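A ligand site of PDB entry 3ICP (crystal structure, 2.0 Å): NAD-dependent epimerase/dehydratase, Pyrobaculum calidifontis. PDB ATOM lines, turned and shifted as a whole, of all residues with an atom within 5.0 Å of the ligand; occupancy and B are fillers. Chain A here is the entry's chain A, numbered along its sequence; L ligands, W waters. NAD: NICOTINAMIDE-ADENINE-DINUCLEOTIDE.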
ATOM      1  N   GLY A   7       4.081  13.989  15.867  1.00  0.00           N
ATOM      2  CA  GLY A   7       5.128  13.064  16.305  1.00  0.00           C
ATOM      3  C   GLY A   7       6.073  13.732  17.301  1.00  0.00           C
ATOM      4  O   GLY A   7       7.182  13.236  17.523  1.00  0.00           O
ATOM      5  N   ALA A   9       6.169  13.625  20.303  1.00  0.00           N
ATOM      6  CA  ALA A   9       6.420  12.827  21.499  1.00  0.00           C
ATOM      7  C   ALA A   9       7.473  11.771  21.188  1.00  0.00           C
ATOM      8  O   ALA A   9       7.819  10.948  22.040  1.00  0.00           O
ATOM      9  CB  ALA A   9       5.123  12.153  21.989  1.00  0.00           C
ATOM     10  N   GLY A  10       7.985  11.784  19.960  1.00  0.00           N
ATOM     11  CA  GLY A  10       8.991  10.807  19.573  1.00  0.00           C
ATOM     12  C   GLY A  10      10.412  11.317  19.724  1.00  0.00           C
ATOM     13  O   GLY A  10      10.642  12.390  20.286  1.00  0.00           O
ATOM     14  N   PHE A  11      11.360  10.528  19.218  1.00  0.00           N
ATOM     15  CA  PHE A  11      12.775  10.863  19.303  1.00  0.00           C
ATOM     16  C   PHE A  11      13.132  12.246  18.756  1.00  0.00           C
ATOM     17  O   PHE A  11      13.360  13.185  19.525  1.00  0.00           O
ATOM     18  CB  PHE A  11      13.585   9.775  18.574  1.00  0.00           C
ATOM     19  CG  PHE A  11      15.062  10.092  18.439  1.00  0.00           C
ATOM     20  CD1 PHE A  11      15.799  10.443  19.558  1.00  0.00           C
ATOM     21  CD2 PHE A  11      15.676  10.065  17.193  1.00  0.00           C
ATOM     22  CE1 PHE A  11      17.150  10.782  19.438  1.00  0.00           C
ATOM     23  CE2 PHE A  11      17.036  10.399  17.069  1.00  0.00           C
ATOM     24  CZ  PHE A  11      17.767  10.763  18.186  1.00  0.00           C
ATOM     25  N   ILE A  12      13.197  12.379  17.434  1.00  0.00           N
ATOM     26  CA  ILE A  12      13.548  13.679  16.860  1.00  0.00           C
ATOM     27  C   ILE A  12      12.541  14.755  17.234  1.00  0.00           C
ATOM     28  O   ILE A  12      12.912  15.871  17.582  1.00  0.00           O
ATOM     29  CB  ILE A  12      13.637  13.613  15.332  1.00  0.00           C
ATOM     30  CG1 ILE A  12      14.708  12.594  14.924  1.00  0.00           C
ATOM     31  CG2 ILE A  12      13.952  14.991  14.774  1.00  0.00           C
ATOM     32  CD1 ILE A  12      14.886  12.471  13.428  1.00  0.00           C
ATOM     33  N   GLY A  13      11.258  14.395  17.156  1.00  0.00           N
ATOM     34  CA  GLY A  13      10.205  15.327  17.477  1.00  0.00           C
ATOM     35  C   GLY A  13      10.267  15.971  18.854  1.00  0.00           C
ATOM     36  O   GLY A  13      10.072  17.170  18.971  1.00  0.00           O
ATOM     37  N   VAL A  30       1.113  16.827  18.534  1.00  0.00           N
ATOM     38  CA  VAL A  30       0.073  15.890  18.146  1.00  0.00           C
ATOM     39  C   VAL A  30       0.788  14.550  17.970  1.00  0.00           C
ATOM     40  O   VAL A  30       1.695  14.437  17.145  1.00  0.00           O
ATOM     41  CB  VAL A  30      -0.610  16.311  16.835  1.00  0.00           C
ATOM     42  CG1 VAL A  30      -1.723  15.337  16.490  1.00  0.00           C
ATOM     43  CG2 VAL A  30      -1.166  17.722  16.993  1.00  0.00           C
ATOM     44  N   ASP A  31       0.381  13.569  18.760  1.00  0.00           N
ATOM     45  CA  ASP A  31       1.033  12.271  18.736  1.00  0.00           C
ATOM     46  C   ASP A  31       0.075  11.194  19.255  1.00  0.00           C
ATOM     47  O   ASP A  31      -0.666  11.421  20.211  1.00  0.00           O
ATOM     48  CB  ASP A  31       2.280  12.355  19.620  1.00  0.00           C
ATOM     49  CG  ASP A  31       3.309  11.296  19.311  1.00  0.00           C
ATOM     50  OD1 ASP A  31       3.034  10.094  19.518  1.00  0.00           O
ATOM     51  OD2 ASP A  31       4.423  11.663  18.868  1.00  0.00           O
ATOM     52  N   ASN A  32       0.102  10.027  18.619  1.00  0.00           N
ATOM     53  CA  ASN A  32      -0.766   8.932  19.023  1.00  0.00           C
ATOM     54  C   ASN A  32      -0.090   8.030  20.044  1.00  0.00           C
ATOM     55  O   ASN A  32      -0.685   7.054  20.515  1.00  0.00           O
ATOM     56  CB  ASN A  32      -1.244   8.143  17.798  1.00  0.00           C
ATOM     57  CG  ASN A  32      -0.187   7.238  17.201  1.00  0.00           C
ATOM     58  OD1 ASN A  32       1.018   7.412  17.414  1.00  0.00           O
ATOM     59  ND2 ASN A  32      -0.629   6.255  16.424  1.00  0.00           N
ATOM     60  N   LEU A  33       1.146   8.373  20.394  1.00  0.00           N
ATOM     61  CA  LEU A  33       1.917   7.638  21.385  1.00  0.00           C
ATOM     62  C   LEU A  33       2.138   6.169  21.040  1.00  0.00           C
ATOM     63  O   LEU A  33       2.229   5.328  21.933  1.00  0.00           O
ATOM     64  CB  LEU A  33       1.241   7.759  22.752  1.00  0.00           C
ATOM     65  CG  LEU A  33       1.019   9.191  23.268  1.00  0.00           C
ATOM     66  CD1 LEU A  33       0.269   9.158  24.612  1.00  0.00           C
ATOM     67  CD2 LEU A  33       2.358   9.903  23.403  1.00  0.00           C
ATOM     68  N   SER A  34       2.219   5.867  19.747  1.00  0.00           N
ATOM     69  CA  SER A  34       2.459   4.503  19.280  1.00  0.00           C
ATOM     70  C   SER A  34       3.923   4.134  19.523  1.00  0.00           C
ATOM     71  O   SER A  34       4.219   3.027  19.965  1.00  0.00           O
ATOM     72  CB  SER A  34       2.115   4.390  17.795  1.00  0.00           C
ATOM     73  OG  SER A  34       2.821   5.357  17.036  1.00  0.00           O
ATOM     74  N   SER A  35       4.843   5.055  19.239  1.00  0.00           N
ATOM     75  CA  SER A  35       6.261   4.812  19.473  1.00  0.00           C
ATOM     76  C   SER A  35       6.864   5.935  20.337  1.00  0.00           C
ATOM     77  O   SER A  35       7.986   5.815  20.812  1.00  0.00           O
ATOM     78  CB  SER A  35       7.030   4.677  18.155  1.00  0.00           C
ATOM     79  OG  SER A  35       6.793   5.774  17.286  1.00  0.00           O
ATOM     80  N   GLY A  36       6.092   6.999  20.537  1.00  0.00           N
ATOM     81  CA  GLY A  36       6.552   8.105  21.355  1.00  0.00           C
ATOM     82  C   GLY A  36       6.082   7.930  22.787  1.00  0.00           C
ATOM     83  O   GLY A  36       5.309   7.009  23.086  1.00  0.00           O
ATOM     84  N   ARG A  50      -3.839  12.329  19.068  1.00  0.00           N
ATOM     85  CA  ARG A  50      -4.659  12.105  17.877  1.00  0.00           C
ATOM     86  C   ARG A  50      -3.923  11.121  16.971  1.00  0.00           C
ATOM     87  O   ARG A  50      -2.701  10.968  17.066  1.00  0.00           O
ATOM     88  CB  ARG A  50      -4.880  13.407  17.093  1.00  0.00           C
ATOM     89  CG  ARG A  50      -5.450  14.604  17.877  1.00  0.00           C
ATOM     90  CD  ARG A  50      -6.922  14.437  18.231  1.00  0.00           C
ATOM     91  NE  ARG A  50      -7.465  15.613  18.923  1.00  0.00           N
ATOM     92  CZ  ARG A  50      -7.915  16.719  18.326  1.00  0.00           C
ATOM     93  NH1 ARG A  50      -7.912  16.847  17.004  1.00  0.00           N
ATOM     94  NH2 ARG A  50      -8.399  17.710  19.077  1.00  0.00           N
ATOM     95  N   ASP A  51      -4.668  10.483  16.057  1.00  0.00           N
ATOM     96  CA  ASP A  51      -4.120   9.523  15.091  1.00  0.00           C
ATOM     97  C   ASP A  51      -4.202  10.127  13.691  1.00  0.00           C
ATOM     98  O   ASP A  51      -5.301  10.297  13.149  1.00  0.00           O
ATOM     99  CB  ASP A  51      -4.920   8.228  15.157  1.00  0.00           C
ATOM    100  CG  ASP A  51      -4.417   7.160  14.183  1.00  0.00           C
ATOM    101  OD1 ASP A  51      -3.422   7.396  13.470  1.00  0.00           O
ATOM    102  OD2 ASP A  51      -5.044   6.076  14.147  1.00  0.00           O
ATOM    103  N   LEU A  52      -3.049  10.450  13.098  1.00  0.00           N
ATOM    104  CA  LEU A  52      -2.995  11.055  11.777  1.00  0.00           C
ATOM    105  C   LEU A  52      -3.636  10.210  10.664  1.00  0.00           C
ATOM    106  O   LEU A  52      -3.943  10.736   9.586  1.00  0.00           O
ATOM    107  CB  LEU A  52      -1.541  11.384  11.410  1.00  0.00           C
ATOM    108  CG  LEU A  52      -1.041  12.797  11.770  1.00  0.00           C
ATOM    109  CD1 LEU A  52      -1.342  13.132  13.222  1.00  0.00           C
ATOM    110  CD2 LEU A  52       0.452  12.882  11.518  1.00  0.00           C
ATOM    111  N   LYS A  53      -3.867   8.924  10.914  1.00  0.00           N
ATOM    112  CA  LYS A  53      -4.510   8.089   9.906  1.00  0.00           C
ATOM    113  C   LYS A  53      -5.979   8.514   9.766  1.00  0.00           C
ATOM    114  O   LYS A  53      -6.648   8.170   8.787  1.00  0.00           O
ATOM    115  CB  LYS A  53      -4.438   6.605  10.286  1.00  0.00           C
ATOM    116  CG  LYS A  53      -3.030   6.002  10.189  1.00  0.00           C
ATOM    117  CD  LYS A  53      -3.070   4.487  10.403  1.00  0.00           C
ATOM    118  CE  LYS A  53      -3.538   4.146  11.810  1.00  0.00           C
ATOM    119  NZ  LYS A  53      -2.680   4.764  12.861  1.00  0.00           N
ATOM    120  N   HIS A  68       5.791  18.144  10.369  1.00  0.00           N
ATOM    121  CA  HIS A  68       5.218  16.812  10.273  1.00  0.00           C
ATOM    122  C   HIS A  68       6.288  15.740  10.403  1.00  0.00           C
ATOM    123  O   HIS A  68       6.902  15.325   9.419  1.00  0.00           O
ATOM    124  CB  HIS A  68       4.476  16.640   8.936  1.00  0.00           C
ATOM    125  CG  HIS A  68       3.855  15.279   8.781  1.00  0.00           C
ATOM    126  ND1 HIS A  68       3.774  14.636   7.570  1.00  0.00           N
ATOM    127  CD2 HIS A  68       3.337  14.431   9.692  1.00  0.00           C
ATOM    128  CE1 HIS A  68       3.240  13.444   7.738  1.00  0.00           C
ATOM    129  NE2 HIS A  68       2.962  13.294   9.017  1.00  0.00           N
ATOM    130  N   PHE A  69       6.502  15.305  11.644  1.00  0.00           N
ATOM    131  CA  PHE A  69       7.519  14.304  11.946  1.00  0.00           C
ATOM    132  C   PHE A  69       6.918  12.975  12.369  1.00  0.00           C
ATOM    133  O   PHE A  69       7.653  12.021  12.643  1.00  0.00           O
ATOM    134  CB  PHE A  69       8.464  14.827  13.043  1.00  0.00           C
ATOM    135  CG  PHE A  69       9.490  15.796  12.537  1.00  0.00           C
ATOM    136  CD1 PHE A  69       9.112  16.923  11.820  1.00  0.00           C
ATOM    137  CD2 PHE A  69      10.858  15.567  12.746  1.00  0.00           C
ATOM    138  CE1 PHE A  69      10.070  17.796  11.292  1.00  0.00           C
ATOM    139  CE2 PHE A  69      11.818  16.434  12.230  1.00  0.00           C
ATOM    140  CZ  PHE A  69      11.419  17.551  11.505  1.00  0.00           C
ATOM    141  N   ALA A  70       5.596  12.909  12.422  1.00  0.00           N
ATOM    142  CA  ALA A  70       4.915  11.673  12.820  1.00  0.00           C
ATOM    143  C   ALA A  70       5.020  10.621  11.739  1.00  0.00           C
ATOM    144  O   ALA A  70       4.882  10.902  10.560  1.00  0.00           O
ATOM    145  CB  ALA A  70       3.436  11.949  13.101  1.00  0.00           C
ATOM    146  N   ALA A  71       5.257   9.382  12.166  1.00  0.00           N
ATOM    147  CA  ALA A  71       5.348   8.220  11.289  1.00  0.00           C
ATOM    148  C   ALA A  71       5.875   7.079  12.107  1.00  0.00           C
ATOM    149  O   ALA A  71       6.378   7.279  13.208  1.00  0.00           O
ATOM    150  CB  ALA A  71       6.290   8.494  10.134  1.00  0.00           C
ATOM    151  N   ASN A  72       5.768   5.863  11.589  1.00  0.00           N
ATOM    152  CA  ASN A  72       6.324   4.750  12.321  1.00  0.00           C
ATOM    153  C   ASN A  72       7.839   4.928  12.191  1.00  0.00           C
ATOM    154  O   ASN A  72       8.319   5.560  11.248  1.00  0.00           O
ATOM    155  CB  ASN A  72       5.847   3.387  11.737  1.00  0.00           C
ATOM    156  CG  ASN A  72       6.083   3.250  10.225  1.00  0.00           C
ATOM    157  OD1 ASN A  72       5.678   4.098   9.433  1.00  0.00           O
ATOM    158  ND2 ASN A  72       6.720   2.149   9.838  1.00  0.00           N
ATOM    159  N   PRO A  73       8.623   4.440  13.169  1.00  0.00           N
ATOM    160  CA  PRO A  73      10.083   4.580  13.132  1.00  0.00           C
ATOM    161  C   PRO A  73      10.706   3.849  11.933  1.00  0.00           C
ATOM    162  O   PRO A  73      10.232   2.794  11.512  1.00  0.00           O
ATOM    163  CB  PRO A  73      10.522   3.994  14.482  1.00  0.00           C
ATOM    164  CG  PRO A  73       9.434   2.983  14.786  1.00  0.00           C
ATOM    165  CD  PRO A  73       8.197   3.764  14.410  1.00  0.00           C
ATOM    166  N   GLU A  74      11.760   4.435  11.383  1.00  0.00           N
ATOM    167  CA  GLU A  74      12.446   3.864  10.235  1.00  0.00           C
ATOM    168  C   GLU A  74      13.420   2.791  10.706  1.00  0.00           C
ATOM    169  O   GLU A  74      14.602   3.070  10.906  1.00  0.00           O
ATOM    170  CB  GLU A  74      13.207   4.969   9.503  1.00  0.00           C
ATOM    171  CG  GLU A  74      14.082   4.499   8.344  1.00  0.00           C
ATOM    172  CD  GLU A  74      14.701   5.678   7.605  1.00  0.00           C
ATOM    173  OE1 GLU A  74      13.929   6.464   7.017  1.00  0.00           O
ATOM    174  OE2 GLU A  74      15.938   5.813   7.610  1.00  0.00           O
ATOM    175  N   GLU A  88       0.755   4.727   7.770  1.00  0.00           N
ATOM    176  CA  GLU A  88       1.435   5.625   8.698  1.00  0.00           C
ATOM    177  C   GLU A  88       2.253   6.714   8.012  1.00  0.00           C
ATOM    178  O   GLU A  88       2.577   7.734   8.614  1.00  0.00           O
ATOM    179  CB  GLU A  88       2.362   4.822   9.627  1.00  0.00           C
ATOM    180  CG  GLU A  88       1.635   3.796  10.503  1.00  0.00           C
ATOM    181  CD  GLU A  88       0.595   4.421  11.421  1.00  0.00           C
ATOM    182  OE1 GLU A  88       0.500   5.658  11.468  1.00  0.00           O
ATOM    183  OE2 GLU A  88      -0.134   3.661  12.093  1.00  0.00           O
ATOM    184  N   ALA A 111       9.438  15.734   7.589  1.00  0.00           N
ATOM    185  CA  ALA A 111      10.605  14.930   7.903  1.00  0.00           C
ATOM    186  C   ALA A 111      10.681  13.799   6.878  1.00  0.00           C
ATOM    187  O   ALA A 111       9.894  12.846   6.932  1.00  0.00           O
ATOM    188  CB  ALA A 111      10.508  14.354   9.321  1.00  0.00           C
ATOM    189  N   SER A 112      11.591  13.908   5.922  1.00  0.00           N
ATOM    190  CA  SER A 112      11.756  12.869   4.922  1.00  0.00           C
ATOM    191  C   SER A 112      12.888  11.942   5.337  1.00  0.00           C
ATOM    192  O   SER A 112      13.247  11.896   6.511  1.00  0.00           O
ATOM    193  CB  SER A 112      12.019  13.470   3.535  1.00  0.00           C
ATOM    194  OG  SER A 112      11.917  12.443   2.560  1.00  0.00           O
ATOM    195  N   SER A 113      13.477  11.221   4.381  1.00  0.00           N
ATOM    196  CA  SER A 113      14.537  10.250   4.696  1.00  0.00           C
ATOM    197  C   SER A 113      15.458   9.957   3.520  1.00  0.00           C
ATOM    198  O   SER A 113      15.049  10.052   2.367  1.00  0.00           O
ATOM    199  CB  SER A 113      13.890   8.939   5.127  1.00  0.00           C
ATOM    200  OG  SER A 113      14.833   7.878   5.251  1.00  0.00           O
ATOM    201  N   TYR A 137       8.743   1.720   2.927  1.00  0.00           N
ATOM    202  CA  TYR A 137       8.898   2.934   3.732  1.00  0.00           C
ATOM    203  C   TYR A 137       9.477   4.058   2.867  1.00  0.00           C
ATOM    204  O   TYR A 137       8.965   5.182   2.864  1.00  0.00           O
ATOM    205  CB  TYR A 137       9.825   2.657   4.902  1.00  0.00           C
ATOM    206  CG  TYR A 137       9.763   3.685   6.005  1.00  0.00           C
ATOM    207  CD1 TYR A 137       8.979   3.481   7.141  1.00  0.00           C
ATOM    208  CD2 TYR A 137      10.534   4.849   5.943  1.00  0.00           C
ATOM    209  CE1 TYR A 137       8.967   4.393   8.186  1.00  0.00           C
ATOM    210  CE2 TYR A 137      10.523   5.785   6.990  1.00  0.00           C
ATOM    211  CZ  TYR A 137       9.740   5.542   8.117  1.00  0.00           C
ATOM    212  OH  TYR A 137       9.766   6.425   9.175  1.00  0.00           O
ATOM    213  N   LYS A 141       7.815   7.658   1.846  1.00  0.00           N
ATOM    214  CA  LYS A 141       8.385   8.972   2.083  1.00  0.00           C
ATOM    215  C   LYS A 141       8.489   9.743   0.770  1.00  0.00           C
ATOM    216  O   LYS A 141       8.201  10.950   0.719  1.00  0.00           O
ATOM    217  CB  LYS A 141       9.766   8.843   2.729  1.00  0.00           C
ATOM    218  CG  LYS A 141       9.728   8.450   4.216  1.00  0.00           C
ATOM    219  CD  LYS A 141       9.043   9.551   5.039  1.00  0.00           C
ATOM    220  CE  LYS A 141       9.185   9.314   6.547  1.00  0.00           C
ATOM    221  NZ  LYS A 141       8.553  10.428   7.336  1.00  0.00           N
ATOM    222  N   TYR A 164      16.543  13.247   6.198  1.00  0.00           N
ATOM    223  CA  TYR A 164      17.468  12.887   7.255  1.00  0.00           C
ATOM    224  C   TYR A 164      18.260  11.622   6.997  1.00  0.00           C
ATOM    225  O   TYR A 164      17.737  10.657   6.451  1.00  0.00           O
ATOM    226  CB  TYR A 164      16.705  12.681   8.573  1.00  0.00           C
ATOM    227  CG  TYR A 164      16.146  13.922   9.202  1.00  0.00           C
ATOM    228  CD1 TYR A 164      16.982  14.885   9.767  1.00  0.00           C
ATOM    229  CD2 TYR A 164      14.764  14.134   9.260  1.00  0.00           C
ATOM    230  CE1 TYR A 164      16.451  16.028  10.380  1.00  0.00           C
ATOM    231  CE2 TYR A 164      14.234  15.260   9.867  1.00  0.00           C
ATOM    232  CZ  TYR A 164      15.084  16.206  10.429  1.00  0.00           C
ATOM    233  OH  TYR A 164      14.530  17.333  11.001  1.00  0.00           O
ATOM    234  N   ALA A 165      19.536  11.629   7.400  1.00  0.00           N
ATOM    235  CA  ALA A 165      20.368  10.425   7.325  1.00  0.00           C
ATOM    236  C   ALA A 165      20.018   9.796   8.676  1.00  0.00           C
ATOM    237  O   ALA A 165      18.872   9.867   9.110  1.00  0.00           O
ATOM    238  CB  ALA A 165      21.847  10.800   7.277  1.00  0.00           C
ATOM    239  N   ASN A 166      20.993   9.184   9.352  1.00  0.00           N
ATOM    240  CA  ASN A 166      20.703   8.592  10.655  1.00  0.00           C
ATOM    241  C   ASN A 166      20.911   9.629  11.772  1.00  0.00           C
ATOM    242  O   ASN A 166      21.946  10.287  11.831  1.00  0.00           O
ATOM    243  CB  ASN A 166      21.567   7.351  10.901  1.00  0.00           C
ATOM    244  CG  ASN A 166      21.166   6.179  10.014  1.00  0.00           C
ATOM    245  OD1 ASN A 166      19.992   6.016   9.683  1.00  0.00           O
ATOM    246  ND2 ASN A 166      22.134   5.351   9.643  1.00  0.00           N
ATOM    247  N   VAL A 167      19.901   9.769  12.633  1.00  0.00           N
ATOM    248  CA  VAL A 167      19.968  10.723  13.738  1.00  0.00           C
ATOM    249  C   VAL A 167      19.976   9.933  15.032  1.00  0.00           C
ATOM    250  O   VAL A 167      19.200   8.988  15.197  1.00  0.00           O
ATOM    251  CB  VAL A 167      18.750  11.683  13.709  1.00  0.00           C
ATOM    252  CG1 VAL A 167      18.847  12.708  14.831  1.00  0.00           C
ATOM    253  CG2 VAL A 167      18.695  12.385  12.377  1.00  0.00           C
ATOM    254  N   HIS A 174      15.014   2.983  19.301  1.00  0.00           N
ATOM    255  CA  HIS A 174      15.083   2.154  18.111  1.00  0.00           C
ATOM    256  C   HIS A 174      16.353   2.458  17.351  1.00  0.00           C
ATOM    257  O   HIS A 174      16.980   3.489  17.551  1.00  0.00           O
ATOM    258  CB  HIS A 174      13.836   2.368  17.239  1.00  0.00           C
ATOM    259  CG  HIS A 174      13.419   3.805  17.104  1.00  0.00           C
ATOM    260  ND1 HIS A 174      13.948   4.647  16.166  1.00  0.00           N
ATOM    261  CD2 HIS A 174      12.547   4.535  17.830  1.00  0.00           C
ATOM    262  CE1 HIS A 174      13.419   5.849  16.299  1.00  0.00           C
ATOM    263  NE2 HIS A 174      12.564   5.810  17.308  1.00  0.00           N
HETATM  264  PA  NAD L   1       9.877   8.000  16.472  1.00  0.00           P
HETATM  265  O1A NAD L   1      10.678   8.180  17.702  1.00  0.00           O
HETATM  266  O2A NAD L   1       9.060   6.771  16.342  1.00  0.00           O
HETATM  267  O5B NAD L   1       8.932   9.289  16.290  1.00  0.00           O
HETATM  268  C5B NAD L   1       7.752   9.230  15.491  1.00  0.00           C
HETATM  269  C4B NAD L   1       6.575   9.832  16.266  1.00  0.00           C
HETATM  270  O4B NAD L   1       5.413   9.808  15.433  1.00  0.00           O
HETATM  271  C3B NAD L   1       6.285   8.960  17.503  1.00  0.00           C
HETATM  272  O3B NAD L   1       6.035   9.757  18.662  1.00  0.00           O
HETATM  273  C2B NAD L   1       5.022   8.219  17.072  1.00  0.00           C
HETATM  274  O2B NAD L   1       4.211   7.910  18.214  1.00  0.00           O
HETATM  275  C1B NAD L   1       4.342   9.304  16.239  1.00  0.00           C
HETATM  276  N9A NAD L   1       3.299   8.728  15.360  1.00  0.00           N
HETATM  277  C8A NAD L   1       3.436   7.652  14.583  1.00  0.00           C
HETATM  278  N7A NAD L   1       2.301   7.433  13.926  1.00  0.00           N
HETATM  279  C5A NAD L   1       1.430   8.367  14.288  1.00  0.00           C
HETATM  280  C6A NAD L   1       0.103   8.627  13.961  1.00  0.00           C
HETATM  281  N6A NAD L   1      -0.566   7.831  13.146  1.00  0.00           N
HETATM  282  N1A NAD L   1      -0.512   9.665  14.551  1.00  0.00           N
HETATM  283  C2A NAD L   1       0.128  10.436  15.415  1.00  0.00           C
HETATM  284  N3A NAD L   1       1.391  10.217  15.739  1.00  0.00           N
HETATM  285  C4A NAD L   1       2.067   9.196  15.193  1.00  0.00           C
HETATM  286  O3  NAD L   1      10.820   8.040  15.162  1.00  0.00           O
HETATM  287  PN  NAD L   1      11.907   9.202  14.876  1.00  0.00           P
HETATM  288  O1N NAD L   1      13.226   8.567  14.647  1.00  0.00           O
HETATM  289  O2N NAD L   1      11.798  10.283  15.877  1.00  0.00           O
HETATM  290  O5D NAD L   1      11.416   9.770  13.441  1.00  0.00           O
HETATM  291  C5D NAD L   1      10.671  10.989  13.352  1.00  0.00           C
HETATM  292  C4D NAD L   1      10.558  11.432  11.896  1.00  0.00           C
HETATM  293  O4D NAD L   1      11.899  11.522  11.391  1.00  0.00           O
HETATM  294  C3D NAD L   1       9.814  10.388  11.057  1.00  0.00           C
HETATM  295  O3D NAD L   1       9.093  10.982   9.982  1.00  0.00           O
HETATM  296  C2D NAD L   1      10.967   9.534  10.521  1.00  0.00           C
HETATM  297  O2D NAD L   1      10.628   8.955   9.262  1.00  0.00           O
HETATM  298  C1D NAD L   1      12.023  10.624  10.279  1.00  0.00           C
HETATM  299  N1N NAD L   1      13.385  10.051  10.148  1.00  0.00           N
HETATM  300  C2N NAD L   1      14.118   9.713  11.292  1.00  0.00           C
HETATM  301  C3N NAD L   1      15.387   9.150  11.149  1.00  0.00           C
HETATM  302  C7N NAD L   1      16.219   8.798  12.387  1.00  0.00           C
HETATM  303  O7N NAD L   1      15.740   8.899  13.519  1.00  0.00           O
HETATM  304  N7N NAD L   1      17.455   8.382  12.149  1.00  0.00           N
HETATM  305  C4N NAD L   1      15.926   8.931   9.894  1.00  0.00           C
HETATM  306  C5N NAD L   1      15.196   9.277   8.745  1.00  0.00           C
HETATM  307  C6N NAD L   1      13.931   9.832   8.877  1.00  0.00           C
HETATM  308  O   HOH W   1       9.777  12.148  16.302  1.00  0.00           O
HETATM  309  O   HOH W   2      18.935   6.487  14.465  1.00  0.00           O
HETATM  310  O   HOH W   3      10.049   7.307  20.330  1.00  0.00           O
HETATM  311  O   HOH W   4       6.813  12.462   9.165  1.00  0.00           O
HETATM  312  O   HOH W   5      17.728   7.699   6.945  1.00  0.00           O
HETATM  313  O   HOH W   6      15.532   5.414  11.828  1.00  0.00           O
HETATM  314  O   HOH W   7       3.000   4.549  13.505  1.00  0.00           O
HETATM  315  O   HOH W   8      13.101   6.624  12.445  1.00  0.00           O
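The backbone NH of Phe 11 is in hydrogen-bond range of an oxygen (O1A) of the ligand, 2.9 Å away.
OD1 of Asp 51 is in hydrogen-bond range of N6A of the ligand (2.9 Å).
A nitrogen (N1A) of the ligand lies within hydrogen-bond range of the backbone NH (N) of Leu 52, at 3.0 Å.
The backbone NH (N) of Ser 34 lies within hydrogen-bond range of an oxygen (O2B) of the ligand (3.2 Å).
O3D of the ligand sits close to O of Phe 69 (3.2 Å).
The side-chain amide oxygen (OD1) of Asn 32 sits close to a nitrogen (N3A) of the ligand, 3.3 Å away.
An oxygen (O2A) of the ligand is in hydrogen-bond range of the side-chain hydroxyl (OG) of Ser 35 (2.7 Å).
O2B of the ligand is in hydrogen-bond range of N of Gly 36, at 3.1 Å.
An oxygen (O1A) of the ligand lies within hydrogen-bond range of a ring nitrogen (NE2) of His 174 (3.1 Å).
The side-chain amino group (NZ) of Lys 141 lies within hydrogen-bond range of an oxygen (O3D) of the ligand, at 2.8 Å.
An oxygen (O2D) of the ligand is in hydrogen-bond range of the side-chain hydroxyl of Tyr 137 (2.7 Å).
OD2 of Asp 31 sits at hydrogen-bond distance from O3B of the ligand, at 2.5 Å.
The side-chain hydroxyl (OG) of Ser 34 sits at hydrogen-bond distance from an oxygen (O2B) of the ligand, 3.1 Å away.
OE1 of Glu 88 is in hydrogen-bond range of N6A of the ligand, 2.9 Å away.
N of Ser 35 is in hydrogen-bond range of O2B of the ligand, at 3.1 Å.
N of Ile 12 is in hydrogen-bond range of O2N of the ligand (3.0 Å).
N of Asn 32 sits at hydrogen-bond distance from N3A of the ligand.
The backbone NH (N) of Gly 10 lies within hydrogen-bond range of an oxygen (O3B) of the ligand, 3.1 Å away.
O4B of the ligand sits at hydrogen-bond distance from N of Ala 71, 3.3 Å away.
The side-chain carboxylate (OE1) of Glu 74 is in hydrogen-bond range of the side-chain hydroxyl (OG) of Ser 113 (2.4 Å).
The side-chain carboxylate (OD1) of Asp 51 lies within salt-bridge range of the side-chain amino group (NZ) of Lys 53, 2.8 Å away.
OD1 of Asn 32 is in hydrogen-bond range of OG of Ser 34.
The side-chain carboxylate (OD1) of Asp 31 lies within hydrogen-bond range of the backbone NH (N) of Leu 33 (2.7 Å).
NZ of Lys 141 sits at hydrogen-bond distance from O of Ala 111 (2.8 Å).
The backbone carbonyl oxygen of Asn 72 lies within hydrogen-bond range of the side-chain hydroxyl of Tyr 137 (2.7 Å).
OE2 of Glu 88 lies within salt-bridge range of NZ of Lys 53 (2.9 Å).
OD2 of Asp 31 is in hydrogen-bond range of N of Ala 9 (3.0 Å).
N of Val 167 lies close to N7N of the ligand.
Residues that only touch the ligand: Gly 7, Ala 9, Leu 33, Arg 50, Lys 53, Ala 70, Pro 73, Glu 74, Ala 111, Ser 112, Ser 113, Tyr 164, Ala 165 and Asn 166.
Water W1 lies within hydrogen-bond range of an oxygen (O2N) of the ligand (2.8 Å), the backbone NH (N) of Gly 13 (2.8 Å) and the backbone carbonyl oxygen (O) of Gly 7 (3.1 Å).
Water W4 lies within hydrogen-bond range of an oxygen (O3D) of the ligand (2.8 Å), the backbone carbonyl oxygen of Ala 70 (2.8 Å), the backbone carbonyl oxygen of His 68 (2.9 Å) and the side-chain amino group of Lys 141 (3.2 Å).
Water W3 lies within hydrogen-bond range of O of Ser 35 and O1A of the ligand.
Water W8 lies within hydrogen-bond range of N of Glu 74 (2.8 Å) and O1N of the ligand (2.9 Å).
Water W7 bridges a nitrogen (N7A) of the ligand (3.0 Å) and the side-chain carboxylate (OE1) of Glu 88 (3.4 Å).
Water W2 bridges O of Val 167 (2.6 Å) and N7N of the ligand (3.3 Å).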
